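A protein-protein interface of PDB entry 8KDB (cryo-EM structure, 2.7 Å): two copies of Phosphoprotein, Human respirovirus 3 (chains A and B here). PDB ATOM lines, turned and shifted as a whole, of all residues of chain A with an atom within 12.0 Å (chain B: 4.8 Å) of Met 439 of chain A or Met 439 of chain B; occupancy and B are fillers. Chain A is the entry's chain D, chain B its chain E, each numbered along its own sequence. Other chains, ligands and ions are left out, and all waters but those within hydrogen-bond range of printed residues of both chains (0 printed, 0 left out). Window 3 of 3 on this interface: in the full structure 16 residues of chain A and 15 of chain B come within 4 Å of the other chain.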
ATOM      1  N   ASP A 435      -5.714 -24.476  -7.722  1.00  0.00           N
ATOM      2  CA  ASP A 435      -5.241 -23.598  -8.784  1.00  0.00           C
ATOM      3  C   ASP A 435      -3.849 -24.018  -9.246  1.00  0.00           C
ATOM      4  O   ASP A 435      -3.573 -24.079 -10.448  1.00  0.00           O
ATOM      5  CB  ASP A 435      -5.229 -22.143  -8.310  1.00  0.00           C
ATOM      6  CG  ASP A 435      -5.201 -21.153  -9.459  1.00  0.00           C
ATOM      7  OD1 ASP A 435      -5.205 -21.591 -10.628  1.00  0.00           O
ATOM      8  OD2 ASP A 435      -5.178 -19.934  -9.191  1.00  0.00           O
ATOM      9  N   LEU A 436      -2.973 -24.308  -8.279  1.00  0.00           N
ATOM     10  CA  LEU A 436      -1.614 -24.722  -8.610  1.00  0.00           C
ATOM     11  C   LEU A 436      -1.609 -26.021  -9.403  1.00  0.00           C
ATOM     12  O   LEU A 436      -0.914 -26.137 -10.421  1.00  0.00           O
ATOM     13  CB  LEU A 436      -0.782 -24.881  -7.337  1.00  0.00           C
ATOM     14  CG  LEU A 436      -0.001 -23.667  -6.835  1.00  0.00           C
ATOM     15  CD1 LEU A 436      -0.931 -22.645  -6.214  1.00  0.00           C
ATOM     16  CD2 LEU A 436       1.055 -24.105  -5.834  1.00  0.00           C
ATOM     17  N   LYS A 437      -2.388 -27.011  -8.960  1.00  0.00           N
ATOM     18  CA  LYS A 437      -2.438 -28.274  -9.686  1.00  0.00           C
ATOM     19  C   LYS A 437      -3.014 -28.083 -11.084  1.00  0.00           C
ATOM     20  O   LYS A 437      -2.479 -28.625 -12.058  1.00  0.00           O
ATOM     21  CB  LYS A 437      -3.249 -29.302  -8.891  1.00  0.00           C
ATOM     22  CG  LYS A 437      -4.636 -28.829  -8.475  1.00  0.00           C
ATOM     23  CD  LYS A 437      -5.317 -29.821  -7.546  1.00  0.00           C
ATOM     24  CE  LYS A 437      -6.624 -29.253  -7.011  1.00  0.00           C
ATOM     25  NZ  LYS A 437      -6.382 -28.055  -6.157  1.00  0.00           N
ATOM     26  N   LYS A 438      -4.090 -27.303 -11.204  1.00  0.00           N
ATOM     27  CA  LYS A 438      -4.704 -27.085 -12.509  1.00  0.00           C
ATOM     28  C   LYS A 438      -3.714 -26.432 -13.464  1.00  0.00           C
ATOM     29  O   LYS A 438      -3.594 -26.838 -14.628  1.00  0.00           O
ATOM     30  CB  LYS A 438      -5.967 -26.236 -12.357  1.00  0.00           C
ATOM     31  CG  LYS A 438      -6.714 -25.995 -13.657  1.00  0.00           C
ATOM     32  CD  LYS A 438      -6.403 -24.622 -14.227  1.00  0.00           C
ATOM     33  CE  LYS A 438      -7.088 -24.410 -15.565  1.00  0.00           C
ATOM     34  NZ  LYS A 438      -6.763 -23.078 -16.149  1.00  0.00           N
ATOM     35  N   MET A 439      -2.983 -25.421 -12.981  1.00  0.00           N
ATOM     36  CA  MET A 439      -1.903 -24.852 -13.778  1.00  0.00           C
ATOM     37  C   MET A 439      -0.888 -25.917 -14.164  1.00  0.00           C
ATOM     38  O   MET A 439      -0.401 -25.936 -15.301  1.00  0.00           O
ATOM     39  CB  MET A 439      -1.212 -23.724 -13.016  1.00  0.00           C
ATOM     40  CG  MET A 439      -0.128 -23.051 -13.828  1.00  0.00           C
ATOM     41  SD  MET A 439       0.668 -21.657 -13.023  1.00  0.00           S
ATOM     42  CE  MET A 439       1.903 -21.276 -14.261  1.00  0.00           C
ATOM     43  N   ASP A 440      -0.555 -26.808 -13.228  1.00  0.00           N
ATOM     44  CA  ASP A 440       0.418 -27.857 -13.510  1.00  0.00           C
ATOM     45  C   ASP A 440      -0.003 -28.688 -14.718  1.00  0.00           C
ATOM     46  O   ASP A 440       0.724 -28.758 -15.717  1.00  0.00           O
ATOM     47  CB  ASP A 440       0.613 -28.742 -12.277  1.00  0.00           C
ATOM     48  CG  ASP A 440       1.868 -29.592 -12.362  1.00  0.00           C
ATOM     49  OD1 ASP A 440       2.437 -29.700 -13.467  1.00  0.00           O
ATOM     50  OD2 ASP A 440       2.290 -30.148 -11.326  1.00  0.00           O
ATOM     51  N   GLU A 441      -1.179 -29.328 -14.654  1.00  0.00           N
ATOM     52  CA  GLU A 441      -1.550 -30.182 -15.790  1.00  0.00           C
ATOM     53  C   GLU A 441      -1.802 -29.374 -17.061  1.00  0.00           C
ATOM     54  O   GLU A 441      -1.481 -29.846 -18.157  1.00  0.00           O
ATOM     55  CB  GLU A 441      -2.747 -31.118 -15.536  1.00  0.00           C
ATOM     56  CG  GLU A 441      -2.566 -32.265 -14.525  1.00  0.00           C
ATOM     57  CD  GLU A 441      -2.783 -31.881 -13.093  1.00  0.00           C
ATOM     58  OE1 GLU A 441      -3.155 -30.732 -12.859  1.00  0.00           O
ATOM     59  OE2 GLU A 441      -2.574 -32.728 -12.201  1.00  0.00           O
ATOM     60  N   SER A 442      -2.373 -28.169 -16.960  1.00  0.00           N
ATOM     61  CA  SER A 442      -2.612 -27.389 -18.173  1.00  0.00           C
ATOM     62  C   SER A 442      -1.302 -27.056 -18.883  1.00  0.00           C
ATOM     63  O   SER A 442      -1.152 -27.296 -20.091  1.00  0.00           O
ATOM     64  CB  SER A 442      -3.382 -26.112 -17.834  1.00  0.00           C
ATOM     65  OG  SER A 442      -2.643 -25.284 -16.953  1.00  0.00           O
ATOM     66  N   HIS A 443      -0.332 -26.516 -18.142  1.00  0.00           N
ATOM     67  CA  HIS A 443       0.936 -26.150 -18.757  1.00  0.00           C
ATOM     68  C   HIS A 443       1.694 -27.382 -19.228  1.00  0.00           C
ATOM     69  O   HIS A 443       2.364 -27.335 -20.264  1.00  0.00           O
ATOM     70  CB  HIS A 443       1.769 -25.322 -17.784  1.00  0.00           C
ATOM     71  CG  HIS A 443       1.287 -23.911 -17.641  1.00  0.00           C
ATOM     72  ND1 HIS A 443       2.128 -22.824 -17.726  1.00  0.00           N
ATOM     73  CD2 HIS A 443       0.045 -23.413 -17.433  1.00  0.00           C
ATOM     74  CE1 HIS A 443       1.425 -21.716 -17.573  1.00  0.00           C
ATOM     75  NE2 HIS A 443       0.159 -22.046 -17.392  1.00  0.00           N
ATOM     76  N   ARG A 444       1.587 -28.500 -18.503  1.00  0.00           N
ATOM     77  CA  ARG A 444       2.214 -29.726 -18.982  1.00  0.00           C
ATOM     78  C   ARG A 444       1.597 -30.179 -20.299  1.00  0.00           C
ATOM     79  O   ARG A 444       2.310 -30.638 -21.197  1.00  0.00           O
ATOM     80  CB  ARG A 444       2.112 -30.831 -17.931  1.00  0.00           C
ATOM     81  CG  ARG A 444       3.006 -30.619 -16.720  1.00  0.00           C
ATOM     82  CD  ARG A 444       2.950 -31.812 -15.781  1.00  0.00           C
ATOM     83  NE  ARG A 444       3.838 -32.885 -16.209  1.00  0.00           N
ATOM     84  CZ  ARG A 444       5.083 -33.040 -15.782  1.00  0.00           C
ATOM     85  NH1 ARG A 444       5.624 -32.203 -14.912  1.00  0.00           N
ATOM     86  NH2 ARG A 444       5.805 -34.059 -16.240  1.00  0.00           N
ATOM     87  N   ARG A 445       0.277 -30.050 -20.438  1.00  0.00           N
ATOM     88  CA  ARG A 445      -0.382 -30.448 -21.679  1.00  0.00           C
ATOM     89  C   ARG A 445       0.078 -29.584 -22.849  1.00  0.00           C
ATOM     90  O   ARG A 445       0.403 -30.098 -23.928  1.00  0.00           O
ATOM     91  CB  ARG A 445      -1.898 -30.366 -21.508  1.00  0.00           C
ATOM     92  CG  ARG A 445      -2.694 -30.982 -22.642  1.00  0.00           C
ATOM     93  CD  ARG A 445      -4.186 -30.875 -22.379  1.00  0.00           C
ATOM     94  NE  ARG A 445      -4.591 -31.660 -21.219  1.00  0.00           N
ATOM     95  CZ  ARG A 445      -5.038 -31.145 -20.082  1.00  0.00           C
ATOM     96  NH1 ARG A 445      -5.153 -29.838 -19.912  1.00  0.00           N
ATOM     97  NH2 ARG A 445      -5.377 -31.961 -19.089  1.00  0.00           N
ATOM     98  N   LEU A 446       0.118 -28.262 -22.652  1.00  0.00           N
ATOM     99  CA  LEU A 446       0.599 -27.398 -23.732  1.00  0.00           C
ATOM    100  C   LEU A 446       2.068 -27.660 -24.058  1.00  0.00           C
ATOM    101  O   LEU A 446       2.455 -27.665 -25.235  1.00  0.00           O
ATOM    102  CB  LEU A 446       0.364 -25.921 -23.405  1.00  0.00           C
ATOM    103  CG  LEU A 446      -1.052 -25.350 -23.590  1.00  0.00           C
ATOM    104  CD1 LEU A 446      -2.062 -25.829 -22.566  1.00  0.00           C
ATOM    105  CD2 LEU A 446      -1.002 -23.829 -23.609  1.00  0.00           C
ATOM    106  N   ILE A 447       2.900 -27.890 -23.040  1.00  0.00           N
ATOM    107  CA  ILE A 447       4.313 -28.155 -23.290  1.00  0.00           C
ATOM    108  C   ILE A 447       4.490 -29.469 -24.042  1.00  0.00           C
ATOM    109  O   ILE A 447       5.345 -29.580 -24.925  1.00  0.00           O
ATOM    110  CB  ILE A 447       5.103 -28.139 -21.968  1.00  0.00           C
ATOM    111  CG1 ILE A 447       5.200 -26.714 -21.426  1.00  0.00           C
ATOM    112  CG2 ILE A 447       6.496 -28.697 -22.172  1.00  0.00           C
ATOM    113  CD1 ILE A 447       5.929 -25.761 -22.345  1.00  0.00           C
ATOM    114  N   GLU A 448       3.684 -30.484 -23.715  1.00  0.00           N
ATOM    115  CA  GLU A 448       3.766 -31.744 -24.446  1.00  0.00           C
ATOM    116  C   GLU A 448       3.277 -31.601 -25.881  1.00  0.00           C
ATOM    117  O   GLU A 448       3.820 -32.251 -26.780  1.00  0.00           O
ATOM    118  CB  GLU A 448       2.983 -32.837 -23.720  1.00  0.00           C
ATOM    119  CG  GLU A 448       3.572 -33.220 -22.374  1.00  0.00           C
ATOM    120  CD  GLU A 448       4.926 -33.889 -22.503  1.00  0.00           C
ATOM    121  OE1 GLU A 448       5.156 -34.583 -23.515  1.00  0.00           O
ATOM    122  OE2 GLU A 448       5.763 -33.716 -21.592  1.00  0.00           O
ATOM    123  N   ASP B 435      -2.507 -12.417  -8.239  1.00  0.00           N
ATOM    124  CA  ASP B 435      -1.160 -12.340  -8.791  1.00  0.00           C
ATOM    125  C   ASP B 435      -0.834 -13.608  -9.575  1.00  0.00           C
ATOM    126  O   ASP B 435      -0.216 -13.551 -10.638  1.00  0.00           O
ATOM    127  CB  ASP B 435      -0.134 -12.124  -7.676  1.00  0.00           C
ATOM    128  CG  ASP B 435       1.184 -11.579  -8.191  1.00  0.00           C
ATOM    129  OD1 ASP B 435       1.396 -11.580  -9.421  1.00  0.00           O
ATOM    130  OD2 ASP B 435       2.012 -11.145  -7.361  1.00  0.00           O
ATOM    131  N   LEU B 436      -1.255 -14.755  -9.038  1.00  0.00           N
ATOM    132  CA  LEU B 436      -1.028 -16.023  -9.722  1.00  0.00           C
ATOM    133  C   LEU B 436      -1.816 -16.090 -11.026  1.00  0.00           C
ATOM    134  O   LEU B 436      -1.354 -16.672 -12.015  1.00  0.00           O
ATOM    135  CB  LEU B 436      -1.393 -17.184  -8.795  1.00  0.00           C
ATOM    136  CG  LEU B 436      -0.995 -18.609  -9.184  1.00  0.00           C
ATOM    137  CD1 LEU B 436      -0.765 -19.433  -7.929  1.00  0.00           C
ATOM    138  CD2 LEU B 436      -2.052 -19.272 -10.057  1.00  0.00           C
ATOM    139  N   LYS B 437      -3.013 -15.501 -11.043  1.00  0.00           N
ATOM    140  CA  LYS B 437      -3.798 -15.464 -12.271  1.00  0.00           C
ATOM    141  C   LYS B 437      -3.065 -14.705 -13.370  1.00  0.00           C
ATOM    142  O   LYS B 437      -3.066 -15.125 -14.533  1.00  0.00           O
ATOM    143  CB  LYS B 437      -5.162 -14.831 -11.998  1.00  0.00           C
ATOM    144  CG  LYS B 437      -6.018 -15.612 -11.015  1.00  0.00           C
ATOM    145  CD  LYS B 437      -7.202 -14.787 -10.530  1.00  0.00           C
ATOM    146  CE  LYS B 437      -6.774 -13.773  -9.480  1.00  0.00           C
ATOM    147  NZ  LYS B 437      -6.300 -14.430  -8.231  1.00  0.00           N
ATOM    148  N   LYS B 438      -2.421 -13.589 -13.016  1.00  0.00           N
ATOM    149  CA  LYS B 438      -1.723 -12.781 -14.012  1.00  0.00           C
ATOM    150  C   LYS B 438      -0.560 -13.548 -14.633  1.00  0.00           C
ATOM    151  O   LYS B 438      -0.394 -13.564 -15.859  1.00  0.00           O
ATOM    152  CB  LYS B 438      -1.230 -11.477 -13.380  1.00  0.00           C
ATOM    153  CG  LYS B 438      -2.279 -10.374 -13.281  1.00  0.00           C
ATOM    154  CD  LYS B 438      -3.289 -10.643 -12.174  1.00  0.00           C
ATOM    155  CE  LYS B 438      -4.254  -9.480 -12.007  1.00  0.00           C
ATOM    156  NZ  LYS B 438      -5.225  -9.719 -10.905  1.00  0.00           N
ATOM    157  N   MET B 439       0.263 -14.186 -13.796  1.00  0.00           N
ATOM    158  CA  MET B 439       1.386 -14.958 -14.318  1.00  0.00           C
ATOM    159  C   MET B 439       0.909 -16.153 -15.137  1.00  0.00           C
ATOM    160  O   MET B 439       1.499 -16.472 -16.177  1.00  0.00           O
ATOM    161  CB  MET B 439       2.306 -15.395 -13.172  1.00  0.00           C
ATOM    162  CG  MET B 439       1.665 -16.282 -12.111  1.00  0.00           C
ATOM    163  SD  MET B 439       1.476 -18.029 -12.527  1.00  0.00           S
ATOM    164  CE  MET B 439       3.173 -18.583 -12.482  1.00  0.00           C
ATOM    165  N   ASP B 440      -0.160 -16.821 -14.692  1.00  0.00           N
ATOM    166  CA  ASP B 440      -0.698 -17.935 -15.466  1.00  0.00           C
ATOM    167  C   ASP B 440      -1.172 -17.471 -16.838  1.00  0.00           C
ATOM    168  O   ASP B 440      -0.889 -18.118 -17.854  1.00  0.00           O
ATOM    169  CB  ASP B 440      -1.839 -18.601 -14.696  1.00  0.00           C
ATOM    170  CG  ASP B 440      -2.036 -20.051 -15.086  1.00  0.00           C
ATOM    171  OD1 ASP B 440      -1.230 -20.567 -15.890  1.00  0.00           O
ATOM    172  OD2 ASP B 440      -2.997 -20.677 -14.591  1.00  0.00           O
ATOM    173  N   GLU B 441      -1.877 -16.337 -16.888  1.00  0.00           N
ATOM    174  CA  GLU B 441      -2.343 -15.801 -18.163  1.00  0.00           C
ATOM    175  C   GLU B 441      -1.175 -15.418 -19.065  1.00  0.00           C
ATOM    176  O   GLU B 441      -1.197 -15.691 -20.273  1.00  0.00           O
ATOM    177  CB  GLU B 441      -3.245 -14.591 -17.919  1.00  0.00           C
ATOM    178  CG  GLU B 441      -4.615 -14.936 -17.362  1.00  0.00           C
ATOM    179  CD  GLU B 441      -5.576 -13.765 -17.420  1.00  0.00           C
ATOM    180  OE1 GLU B 441      -5.261 -12.771 -18.107  1.00  0.00           O
ATOM    181  OE2 GLU B 441      -6.644 -13.838 -16.777  1.00  0.00           O
ATOM    182  N   SER B 442      -0.152 -14.777 -18.498  1.00  0.00           N
ATOM    183  CA  SER B 442       1.006 -14.375 -19.292  1.00  0.00           C
ATOM    184  C   SER B 442       1.709 -15.589 -19.884  1.00  0.00           C
ATOM    185  O   SER B 442       2.060 -15.604 -21.072  1.00  0.00           O
ATOM    186  CB  SER B 442       1.969 -13.558 -18.429  1.00  0.00           C
ATOM    187  OG  SER B 442       3.122 -13.181 -19.161  1.00  0.00           O
ATOM    188  N   HIS B 443       1.912 -16.627 -19.070  1.00  0.00           N
ATOM    189  CA  HIS B 443       2.567 -17.832 -19.566  1.00  0.00           C
ATOM    190  C   HIS B 443       1.725 -18.518 -20.633  1.00  0.00           C
ATOM    191  O   HIS B 443       2.261 -19.014 -21.630  1.00  0.00           O
ATOM    192  CB  HIS B 443       2.862 -18.785 -18.409  1.00  0.00           C
ATOM    193  CG  HIS B 443       3.821 -18.233 -17.401  1.00  0.00           C
ATOM    194  ND1 HIS B 443       4.544 -17.079 -17.616  1.00  0.00           N
ATOM    195  CD2 HIS B 443       4.176 -18.677 -16.172  1.00  0.00           C
ATOM    196  CE1 HIS B 443       5.303 -16.835 -16.562  1.00  0.00           C
ATOM    197  NE2 HIS B 443       5.099 -17.790 -15.672  1.00  0.00           N
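Of chain B, only Met 439 (3.5 Å), Asp 440 (3.4 Å) and His 443 (3.9 Å) come within 4 Å of Met 439 of chain A.
Met 439 of chain B touches just one residue of chain A: Met 439.
No residue of chain A comes within 4 Å of Asp 435 of chain B.
Leu 436 of chain B touches just these residues of chain A: Asp 435 and Leu 436.
No residue of chain A comes within 4 Å of Lys 438 of chain B.
Asp 440 of chain B touches just these residues of chain A: Met 439 (3.4 Å) and His 443 (2.5 Å).
No residue of chain A comes within 4 Å of Glu 441 of chain B.
No residue of chain A comes within 4 Å of Ser 442 of chain B.
Of the printed residues of chain A, His 443 of chain B touches Met 439 (3.9 Å) and His 443 (3.4 Å).
Of the printed residues of chain B, Leu 436 of chain A touches Leu 436.
Of the printed residues of chain B, Asp 435 of chain A touches Leu 436 (3.3 Å).
Printed residues of chain B within 4 Å of His 443 of chain A: Asp 440 and His 443.
Glu 441 of chain A touches none of the printed residues of chain B.
Arg 445 of chain A touches none of the printed residues of chain B.
The nearest residue of chain B that does not touch Met 439 of chain A is Leu 436 of chain B (4.7 Å).
The nearest residue of chain A that does not touch Met 439 of chain B is His 443 of chain A (5.4 Å).
Printed residues of chain A that touch a printed residue of chain B: Asp 435, Leu 436, Met 439 and His 443.
Hydrophobic or aromatic side chains of chain A that line the printed part of chain B: Leu 436, Met 439 and His 443.
Asp 435 of chain A touches Leu 436 of chain B.
CD1 of Leu 436 of chain B touches CD1 of Leu 436 of chain A, at 3.6 Å.
CD2 of His 443 of chain B touches CE of Met 439 of chain A, at 3.9 Å.
CB of His 443 of chain B touches CE1 of His 443 of chain A, at 3.4 Å.
Asp 435 of chain A touches Leu 436 of chain B, but with the chains exchanged Leu 436 of chain A does not touch Asp 435 of chain B (9.6 Å).
Met 439 of chain A touches its own counterpart, Met 439 of chain B.
Met 439 of chain A touches Asp 440 of chain B, but with the chains exchanged Asp 440 of chain A does not touch Met 439 of chain B (9.0 Å).
Met 439 of chain A touches His 443 of chain B, but with the chains exchanged His 443 of chain A does not touch Met 439 of chain B (5.4 Å).
9 positions are printed for both chains.
Of the 7 pairs that touch across the chains among the printed residues, 3 have their exchanged pair printed and touching as well.
The backbone carbonyl oxygen of Met 439 of chain B sits close to a ring nitrogen (ND1) of His 443 of chain B (3.4 Å).
OG of Ser 442 of chain A is in hydrogen-bond range of O of Met 439 of chain A (2.9 Å).
OD1 of Asp 440 of chain B lies close to SD of Met 439 of chain A (3.6 Å).
SD of Met 439 of chain A lies close to SD of Met 439 of chain B (3.7 Å).
A ring nitrogen (NE2) of His 443 of chain A is in hydrogen-bond range of the side-chain carboxylate (OD1) of Asp 440 of chain B (2.5 Å).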
